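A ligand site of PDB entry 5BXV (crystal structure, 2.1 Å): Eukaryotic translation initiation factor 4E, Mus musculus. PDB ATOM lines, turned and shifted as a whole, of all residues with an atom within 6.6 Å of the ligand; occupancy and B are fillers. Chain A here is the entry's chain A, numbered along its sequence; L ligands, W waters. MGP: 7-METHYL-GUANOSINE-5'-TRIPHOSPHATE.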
ATOM      1  N   PHE A  23       3.870   9.155   5.990  1.00  0.00           N
ATOM      2  CA  PHE A  23       3.032   9.928   6.918  1.00  0.00           C
ATOM      3  C   PHE A  23       3.901  10.704   7.908  1.00  0.00           C
ATOM      4  O   PHE A  23       4.626  10.118   8.719  1.00  0.00           O
ATOM      5  CB  PHE A  23       2.060   9.040   7.720  1.00  0.00           C
ATOM      6  CG  PHE A  23       1.127   9.805   8.629  1.00  0.00           C
ATOM      7  CD1 PHE A  23       1.484  10.096   9.919  1.00  0.00           C
ATOM      8  CD2 PHE A  23      -0.116  10.241   8.166  1.00  0.00           C
ATOM      9  CE1 PHE A  23       0.635  10.795  10.766  1.00  0.00           C
ATOM     10  CE2 PHE A  23      -0.977  10.934   9.017  1.00  0.00           C
ATOM     11  CZ  PHE A  23      -0.592  11.205  10.314  1.00  0.00           C
ATOM     12  N   TRP A  31      -5.237  14.039   9.579  1.00  0.00           N
ATOM     13  CA  TRP A  31      -4.540  12.793   9.330  1.00  0.00           C
ATOM     14  C   TRP A  31      -4.335  12.636   7.827  1.00  0.00           C
ATOM     15  O   TRP A  31      -3.209  12.468   7.368  1.00  0.00           O
ATOM     16  CB  TRP A  31      -5.288  11.595   9.945  1.00  0.00           C
ATOM     17  CG  TRP A  31      -4.537  10.278   9.765  1.00  0.00           C
ATOM     18  CD1 TRP A  31      -3.634   9.725  10.625  1.00  0.00           C
ATOM     19  CD2 TRP A  31      -4.617   9.379   8.649  1.00  0.00           C
ATOM     20  NE1 TRP A  31      -3.157   8.536  10.112  1.00  0.00           N
ATOM     21  CE2 TRP A  31      -3.748   8.306   8.900  1.00  0.00           C
ATOM     22  CE3 TRP A  31      -5.348   9.381   7.456  1.00  0.00           C
ATOM     23  CZ2 TRP A  31      -3.583   7.254   8.008  1.00  0.00           C
ATOM     24  CZ3 TRP A  31      -5.187   8.315   6.581  1.00  0.00           C
ATOM     25  CH2 TRP A  31      -4.313   7.286   6.858  1.00  0.00           C
ATOM     26  N   GLN A  32      -5.389  12.739   7.034  1.00  0.00           N
ATOM     27  CA  GLN A  32      -5.210  12.597   5.592  1.00  0.00           C
ATOM     28  C   GLN A  32      -4.246  13.625   5.017  1.00  0.00           C
ATOM     29  O   GLN A  32      -3.515  13.322   4.089  1.00  0.00           O
ATOM     30  CB  GLN A  32      -6.543  12.677   4.846  1.00  0.00           C
ATOM     31  CG  GLN A  32      -6.370  12.248   3.386  1.00  0.00           C
ATOM     32  CD  GLN A  32      -7.644  12.240   2.572  1.00  0.00           C
ATOM     33  OE1 GLN A  32      -8.695  12.685   3.040  1.00  0.00           O
ATOM     34  NE2 GLN A  32      -7.574  11.729   1.348  1.00  0.00           N
ATOM     35  N   GLY A  63       5.793   8.913  15.569  1.00  0.00           N
ATOM     36  CA  GLY A  63       4.516   9.247  14.975  1.00  0.00           C
ATOM     37  C   GLY A  63       4.454   9.179  13.455  1.00  0.00           C
ATOM     38  O   GLY A  63       3.388   9.345  12.865  1.00  0.00           O
ATOM     39  N   ASP A  65       4.914   7.280   9.615  1.00  0.00           N
ATOM     40  CA  ASP A  65       4.737   5.960   8.965  1.00  0.00           C
ATOM     41  C   ASP A  65       5.330   5.838   7.564  1.00  0.00           C
ATOM     42  O   ASP A  65       5.438   6.831   6.840  1.00  0.00           O
ATOM     43  CB  ASP A  65       3.266   5.569   8.777  1.00  0.00           C
ATOM     44  CG  ASP A  65       2.360   5.948   9.911  1.00  0.00           C
ATOM     45  OD1 ASP A  65       2.728   5.868  11.100  1.00  0.00           O
ATOM     46  OD2 ASP A  65       1.198   6.243   9.586  1.00  0.00           O
ATOM     47  N   PRO A  75      -3.701   4.357   1.379  1.00  0.00           N
ATOM     48  CA  PRO A  75      -3.413   3.617   2.615  1.00  0.00           C
ATOM     49  C   PRO A  75      -4.273   4.058   3.797  1.00  0.00           C
ATOM     50  O   PRO A  75      -3.769   4.450   4.864  1.00  0.00           O
ATOM     51  CB  PRO A  75      -1.935   3.929   2.851  1.00  0.00           C
ATOM     52  CG  PRO A  75      -1.772   5.319   2.286  1.00  0.00           C
ATOM     53  CD  PRO A  75      -2.683   5.382   1.093  1.00  0.00           C
ATOM     54  N   MET A  76      -5.590   4.016   3.593  1.00  0.00           N
ATOM     55  CA  MET A  76      -6.493   4.429   4.626  1.00  0.00           C
ATOM     56  C   MET A  76      -7.729   3.520   4.621  1.00  0.00           C
ATOM     57  O   MET A  76      -8.074   2.921   3.594  1.00  0.00           O
ATOM     58  CB  MET A  76      -6.891   5.902   4.403  1.00  0.00           C
ATOM     59  CG  MET A  76      -7.449   6.187   3.049  1.00  0.00           C
ATOM     60  SD  MET A  76      -7.941   7.938   2.721  1.00  0.00           S
ATOM     61  CE  MET A  76      -6.351   8.707   2.641  1.00  0.00           C
ATOM     62  N   TRP A  77      -8.363   3.437   5.779  1.00  0.00           N
ATOM     63  CA  TRP A  77      -9.558   2.614   5.994  1.00  0.00           C
ATOM     64  C   TRP A  77     -10.654   2.876   4.951  1.00  0.00           C
ATOM     65  O   TRP A  77     -11.291   1.960   4.451  1.00  0.00           O
ATOM     66  CB  TRP A  77     -10.163   2.888   7.367  1.00  0.00           C
ATOM     67  CG  TRP A  77      -9.272   2.741   8.528  1.00  0.00           C
ATOM     68  CD1 TRP A  77      -8.264   1.805   8.707  1.00  0.00           C
ATOM     69  CD2 TRP A  77      -9.282   3.549   9.704  1.00  0.00           C
ATOM     70  NE1 TRP A  77      -7.673   1.989   9.929  1.00  0.00           N
ATOM     71  CE2 TRP A  77      -8.278   3.053  10.555  1.00  0.00           C
ATOM     72  CE3 TRP A  77     -10.052   4.635  10.123  1.00  0.00           C
ATOM     73  CZ2 TRP A  77      -8.025   3.622  11.804  1.00  0.00           C
ATOM     74  CZ3 TRP A  77      -9.796   5.196  11.349  1.00  0.00           C
ATOM     75  CH2 TRP A  77      -8.789   4.693  12.176  1.00  0.00           C
ATOM     76  N   GLU A  78     -10.834   4.151   4.626  1.00  0.00           N
ATOM     77  CA  GLU A  78     -11.919   4.599   3.762  1.00  0.00           C
ATOM     78  C   GLU A  78     -11.847   4.133   2.317  1.00  0.00           C
ATOM     79  O   GLU A  78     -12.858   4.134   1.636  1.00  0.00           O
ATOM     80  CB  GLU A  78     -11.973   6.131   3.774  1.00  0.00           C
ATOM     81  CG  GLU A  78     -12.364   6.691   5.137  1.00  0.00           C
ATOM     82  CD  GLU A  78     -11.177   6.976   6.084  1.00  0.00           C
ATOM     83  OE1 GLU A  78     -10.035   6.458   5.890  1.00  0.00           O
ATOM     84  OE2 GLU A  78     -11.404   7.727   7.055  1.00  0.00           O
ATOM     85  N   ARG A  87      -6.198  -6.117   9.059  1.00  0.00           N
ATOM     86  CA  ARG A  87      -4.729  -6.251   9.063  1.00  0.00           C
ATOM     87  C   ARG A  87      -4.198  -7.366   9.968  1.00  0.00           C
ATOM     88  O   ARG A  87      -4.761  -7.629  11.037  1.00  0.00           O
ATOM     89  CB  ARG A  87      -4.061  -4.952   9.528  1.00  0.00           C
ATOM     90  CG  ARG A  87      -4.467  -4.551  10.974  1.00  0.00           C
ATOM     91  CD  ARG A  87      -3.855  -3.217  11.381  1.00  0.00           C
ATOM     92  NE  ARG A  87      -4.249  -2.823  12.740  1.00  0.00           N
ATOM     93  CZ  ARG A  87      -3.809  -1.721  13.357  1.00  0.00           C
ATOM     94  NH1 ARG A  87      -4.207  -1.440  14.605  1.00  0.00           N
ATOM     95  NH2 ARG A  87      -2.955  -0.905  12.744  1.00  0.00           N
ATOM     96  N   VAL A 128       1.982  -1.506   6.211  1.00  0.00           N
ATOM     97  CA  VAL A 128       2.163  -0.268   6.940  1.00  0.00           C
ATOM     98  C   VAL A 128       3.149  -0.504   8.104  1.00  0.00           C
ATOM     99  O   VAL A 128       2.979  -1.456   8.913  1.00  0.00           O
ATOM    100  CB  VAL A 128       0.815   0.271   7.537  1.00  0.00           C
ATOM    101  CG1 VAL A 128       1.041   1.583   8.283  1.00  0.00           C
ATOM    102  CG2 VAL A 128      -0.258   0.482   6.443  1.00  0.00           C
ATOM    103  N   ASN A 130       4.338   1.683  11.415  1.00  0.00           N
ATOM    104  CA  ASN A 130       4.082   2.787  12.373  1.00  0.00           C
ATOM    105  C   ASN A 130       5.212   2.887  13.367  1.00  0.00           C
ATOM    106  O   ASN A 130       5.382   1.978  14.206  1.00  0.00           O
ATOM    107  CB  ASN A 130       2.816   2.559  13.176  1.00  0.00           C
ATOM    108  CG  ASN A 130       1.558   2.386  12.322  1.00  0.00           C
ATOM    109  OD1 ASN A 130       0.848   1.396  12.453  1.00  0.00           O
ATOM    110  ND2 ASN A 130       1.242   3.390  11.529  1.00  0.00           N
ATOM    111  N   ARG A 132       6.454   4.410  16.612  1.00  0.00           N
ATOM    112  CA  ARG A 132       5.740   4.918  17.783  1.00  0.00           C
ATOM    113  C   ARG A 132       6.551   4.754  19.085  1.00  0.00           C
ATOM    114  O   ARG A 132       7.177   3.739  19.298  1.00  0.00           O
ATOM    115  CB  ARG A 132       4.387   4.203  17.964  1.00  0.00           C
ATOM    116  CG  ARG A 132       3.386   4.397  16.817  1.00  0.00           C
ATOM    117  CD  ARG A 132       2.974   5.859  16.651  1.00  0.00           C
ATOM    118  NE  ARG A 132       1.964   6.042  15.575  1.00  0.00           N
ATOM    119  CZ  ARG A 132       2.207   6.181  14.273  1.00  0.00           C
ATOM    120  NH1 ARG A 132       3.447   6.202  13.769  1.00  0.00           N
ATOM    121  NH2 ARG A 132       1.175   6.321  13.432  1.00  0.00           N
ATOM    122  N   LYS A 134       5.333   4.224  22.067  1.00  0.00           N
ATOM    123  CA  LYS A 134       4.754   3.122  22.835  1.00  0.00           C
ATOM    124  C   LYS A 134       5.022   1.733  22.258  1.00  0.00           C
ATOM    125  O   LYS A 134       4.747   0.728  22.898  1.00  0.00           O
ATOM    126  CB  LYS A 134       3.237   3.320  22.964  1.00  0.00           C
ATOM    127  CG  LYS A 134       2.861   4.625  23.674  1.00  0.00           C
ATOM    128  CD  LYS A 134       1.361   4.767  23.882  1.00  0.00           C
ATOM    129  CE  LYS A 134       0.872   3.994  25.093  1.00  0.00           C
ATOM    130  NZ  LYS A 134       1.421   4.529  26.376  1.00  0.00           N
ATOM    131  N   GLY A 135       5.557   1.667  21.039  1.00  0.00           N
ATOM    132  CA  GLY A 135       5.876   0.392  20.437  1.00  0.00           C
ATOM    133  C   GLY A 135       5.574   0.387  18.960  1.00  0.00           C
ATOM    134  O   GLY A 135       4.452   0.709  18.537  1.00  0.00           O
ATOM    135  N   LYS A 137       4.844  -0.710  15.119  1.00  0.00           N
ATOM    136  CA  LYS A 137       3.910  -1.701  14.555  1.00  0.00           C
ATOM    137  C   LYS A 137       4.171  -1.946  13.083  1.00  0.00           C
ATOM    138  O   LYS A 137       4.442  -1.020  12.329  1.00  0.00           O
ATOM    139  CB  LYS A 137       2.463  -1.236  14.755  1.00  0.00           C
ATOM    140  CG  LYS A 137       2.021  -1.174  16.234  1.00  0.00           C
ATOM    141  CD  LYS A 137       0.614  -0.573  16.366  1.00  0.00           C
ATOM    142  CE  LYS A 137       0.664   0.949  16.396  1.00  0.00           C
ATOM    143  NZ  LYS A 137      -0.632   1.610  16.546  1.00  0.00           N
ATOM    144  N   TRP A 141      -2.197  -5.296   5.287  1.00  0.00           N
ATOM    145  CA  TRP A 141      -3.591  -4.977   5.087  1.00  0.00           C
ATOM    146  C   TRP A 141      -4.161  -5.870   3.984  1.00  0.00           C
ATOM    147  O   TRP A 141      -3.573  -5.984   2.930  1.00  0.00           O
ATOM    148  CB  TRP A 141      -3.748  -3.507   4.682  1.00  0.00           C
ATOM    149  CG  TRP A 141      -3.596  -2.529   5.783  1.00  0.00           C
ATOM    150  CD1 TRP A 141      -2.809  -2.665   6.904  1.00  0.00           C
ATOM    151  CD2 TRP A 141      -4.255  -1.263   5.897  1.00  0.00           C
ATOM    152  NE1 TRP A 141      -2.941  -1.556   7.714  1.00  0.00           N
ATOM    153  CE2 TRP A 141      -3.832  -0.679   7.108  1.00  0.00           C
ATOM    154  CE3 TRP A 141      -5.161  -0.573   5.097  1.00  0.00           C
ATOM    155  CZ2 TRP A 141      -4.277   0.577   7.530  1.00  0.00           C
ATOM    156  CZ3 TRP A 141      -5.615   0.671   5.501  1.00  0.00           C
ATOM    157  CH2 TRP A 141      -5.171   1.242   6.705  1.00  0.00           C
ATOM    158  N   THR A 178     -10.909  -1.453  14.507  1.00  0.00           N
ATOM    159  CA  THR A 178      -9.873  -0.467  14.810  1.00  0.00           C
ATOM    160  C   THR A 178     -10.450   0.952  14.878  1.00  0.00           C
ATOM    161  O   THR A 178     -10.176   1.704  15.808  1.00  0.00           O
ATOM    162  CB  THR A 178      -8.729  -0.493  13.773  1.00  0.00           C
ATOM    163  OG1 THR A 178      -8.166  -1.797  13.710  1.00  0.00           O
ATOM    164  CG2 THR A 178      -7.634   0.527  14.121  1.00  0.00           C
ATOM    165  N   LYS A 181     -12.613   1.447  18.201  1.00  0.00           N
ATOM    166  CA  LYS A 181     -11.754   1.605  19.369  1.00  0.00           C
ATOM    167  C   LYS A 181     -10.806   2.805  19.216  1.00  0.00           C
ATOM    168  O   LYS A 181     -11.059   3.726  18.437  1.00  0.00           O
ATOM    169  CB  LYS A 181     -10.953   0.315  19.597  1.00  0.00           C
ATOM    170  CG  LYS A 181     -11.812  -0.952  19.722  1.00  0.00           C
ATOM    171  CD  LYS A 181     -10.948  -2.210  19.807  1.00  0.00           C
ATOM    172  CE  LYS A 181     -11.787  -3.489  19.813  1.00  0.00           C
ATOM    173  NZ  LYS A 181     -10.963  -4.725  19.933  1.00  0.00           N
HETATM  174  PA  MGP L   1      -2.465   5.146  14.368  1.00  0.00           P
HETATM  175  O1A MGP L   1      -2.630   4.133  13.229  1.00  0.00           O
HETATM  176  O2A MGP L   1      -1.433   6.148  13.936  1.00  0.00           O
HETATM  177  O3A MGP L   1      -2.131   4.448  15.736  1.00  0.00           O
HETATM  178  O5' MGP L   1      -3.837   5.900  14.569  1.00  0.00           O
HETATM  179  PB  MGP L   1      -1.454   5.167  16.978  1.00  0.00           P
HETATM  180  O1B MGP L   1      -0.930   6.558  16.617  1.00  0.00           O
HETATM  181  O2B MGP L   1      -0.286   4.304  17.388  1.00  0.00           O
HETATM  182  O3B MGP L   1      -2.466   5.327  18.163  1.00  0.00           O
HETATM  183  PC  MGP L   1      -3.606   4.302  18.454  1.00  0.00           P
HETATM  184  O1C MGP L   1      -4.887   4.762  17.793  1.00  0.00           O
HETATM  185  O2C MGP L   1      -3.809   4.207  19.942  1.00  0.00           O
HETATM  186  O3C MGP L   1      -3.219   2.931  17.909  1.00  0.00           O
HETATM  187  C5' MGP L   1      -3.964   7.142  15.173  1.00  0.00           C
HETATM  188  C4' MGP L   1      -5.073   8.013  14.621  1.00  0.00           C
HETATM  189  O4' MGP L   1      -4.796   8.550  13.357  1.00  0.00           O
HETATM  190  C3' MGP L   1      -6.373   7.239  14.405  1.00  0.00           C
HETATM  191  O3' MGP L   1      -7.088   7.021  15.547  1.00  0.00           O
HETATM  192  C2' MGP L   1      -7.087   8.065  13.455  1.00  0.00           C
HETATM  193  O2' MGP L   1      -7.552   9.219  14.040  1.00  0.00           O
HETATM  194  C1' MGP L   1      -5.967   8.361  12.511  1.00  0.00           C
HETATM  195  N9  MGP L   1      -5.887   7.339  11.481  1.00  0.00           N
HETATM  196  C8  MGP L   1      -4.909   6.215  11.404  1.00  0.00           C
HETATM  197  N7  MGP L   1      -5.344   5.485  10.169  1.00  0.00           N
HETATM  198  CM7 MGP L   1      -4.645   4.297   9.669  1.00  0.00           C
HETATM  199  C5  MGP L   1      -6.467   6.184   9.618  1.00  0.00           C
HETATM  200  C6  MGP L   1      -7.298   5.921   8.410  1.00  0.00           C
HETATM  201  O6  MGP L   1      -7.080   4.979   7.649  1.00  0.00           O
HETATM  202  N1  MGP L   1      -8.382   6.818   8.155  1.00  0.00           N
HETATM  203  C2  MGP L   1      -8.718   7.942   8.975  1.00  0.00           C
HETATM  204  N2  MGP L   1      -9.841   8.859   8.688  1.00  0.00           N
HETATM  205  N3  MGP L   1      -7.897   8.194  10.143  1.00  0.00           N
HETATM  206  C4  MGP L   1      -6.795   7.290  10.436  1.00  0.00           C
HETATM  207  O   HOH W   1      -1.547   8.645  13.271  1.00  0.00           O
HETATM  208  O   HOH W   2      -1.054   6.547  11.054  1.00  0.00           O
HETATM  209  O   HOH W   3      -6.599   3.860  15.830  1.00  0.00           O
HETATM  210  O   HOH W   4       1.120   4.108  19.663  1.00  0.00           O
HETATM  211  O   HOH W   5      -3.619   0.912  16.007  1.00  0.00           O
HETATM  212  O   HOH W   6      -4.938   2.621  13.697  1.00  0.00           O
HETATM  213  O   HOH W   7      -2.894  10.900  14.727  1.00  0.00           O
HETATM  214  O   HOH W   8      -1.495   4.262   9.093  1.00  0.00           O
HETATM  215  O   HOH W   9      -1.442   1.340  13.701  1.00  0.00           O
HETATM  216  O   HOH W  10      -2.492   1.956  10.721  1.00  0.00           O
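An oxygen (O2A) of the ligand is in salt-bridge range of the guanidinium group (NH2) of Arg 132, at 2.7 Å. A nitrogen (N2) of the ligand lies within hydrogen-bond range of the side-chain carboxylate of Glu 78 (2.5 Å). N of Trp 77 lies within hydrogen-bond range of O6 of the ligand (2.7 Å). The side-chain amino group of Lys 137 lies within salt-bridge range of an oxygen (O2B) of the ligand (2.8 Å).
The backbone carbonyl oxygen (O) of Lys 137 sits at hydrogen-bond distance from the backbone NH (N) of Asn 130 (2.9 Å). The guanidinium group (NH1) of Arg 132 lies within salt-bridge range of the side-chain carboxylate (OD1) of Asp 65. The guanidinium group (NH1) of Arg 132 lies close to the backbone carbonyl oxygen (O) of Gly 63 (3.3 Å). NH2 of Arg 132 sits close to ND2 of Asn 130, at 3.5 Å.
A nitrogen (N9) of the ligand sits close to the indole nitrogen (NE1) of Trp 31. Residues that only touch the ligand: Met 76. Within 4 Å of the ligand: Trp 31, Met 76, Trp 77, Glu 78, Arg 132 and Lys 137.
Water W5 lies within hydrogen-bond range of the guanidinium group (NH1) of Arg 87, an oxygen (O3C) of the ligand and the side-chain amino group (NZ) of Lys 137. Water W2 lies within hydrogen-bond range of OD2 of Asp 65 (2.7 Å), O2A of the ligand (2.9 Å), NE1 of Trp 31 (3.0 Å) and NH2 of Arg 132 (3.3 Å). Water W9 lies within hydrogen-bond range of OD1 of Asn 130 (2.6 Å), NH2 of Arg 87 (2.9 Å), NZ of Lys 137 (3.0 Å) and O1A of the ligand (3.1 Å).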
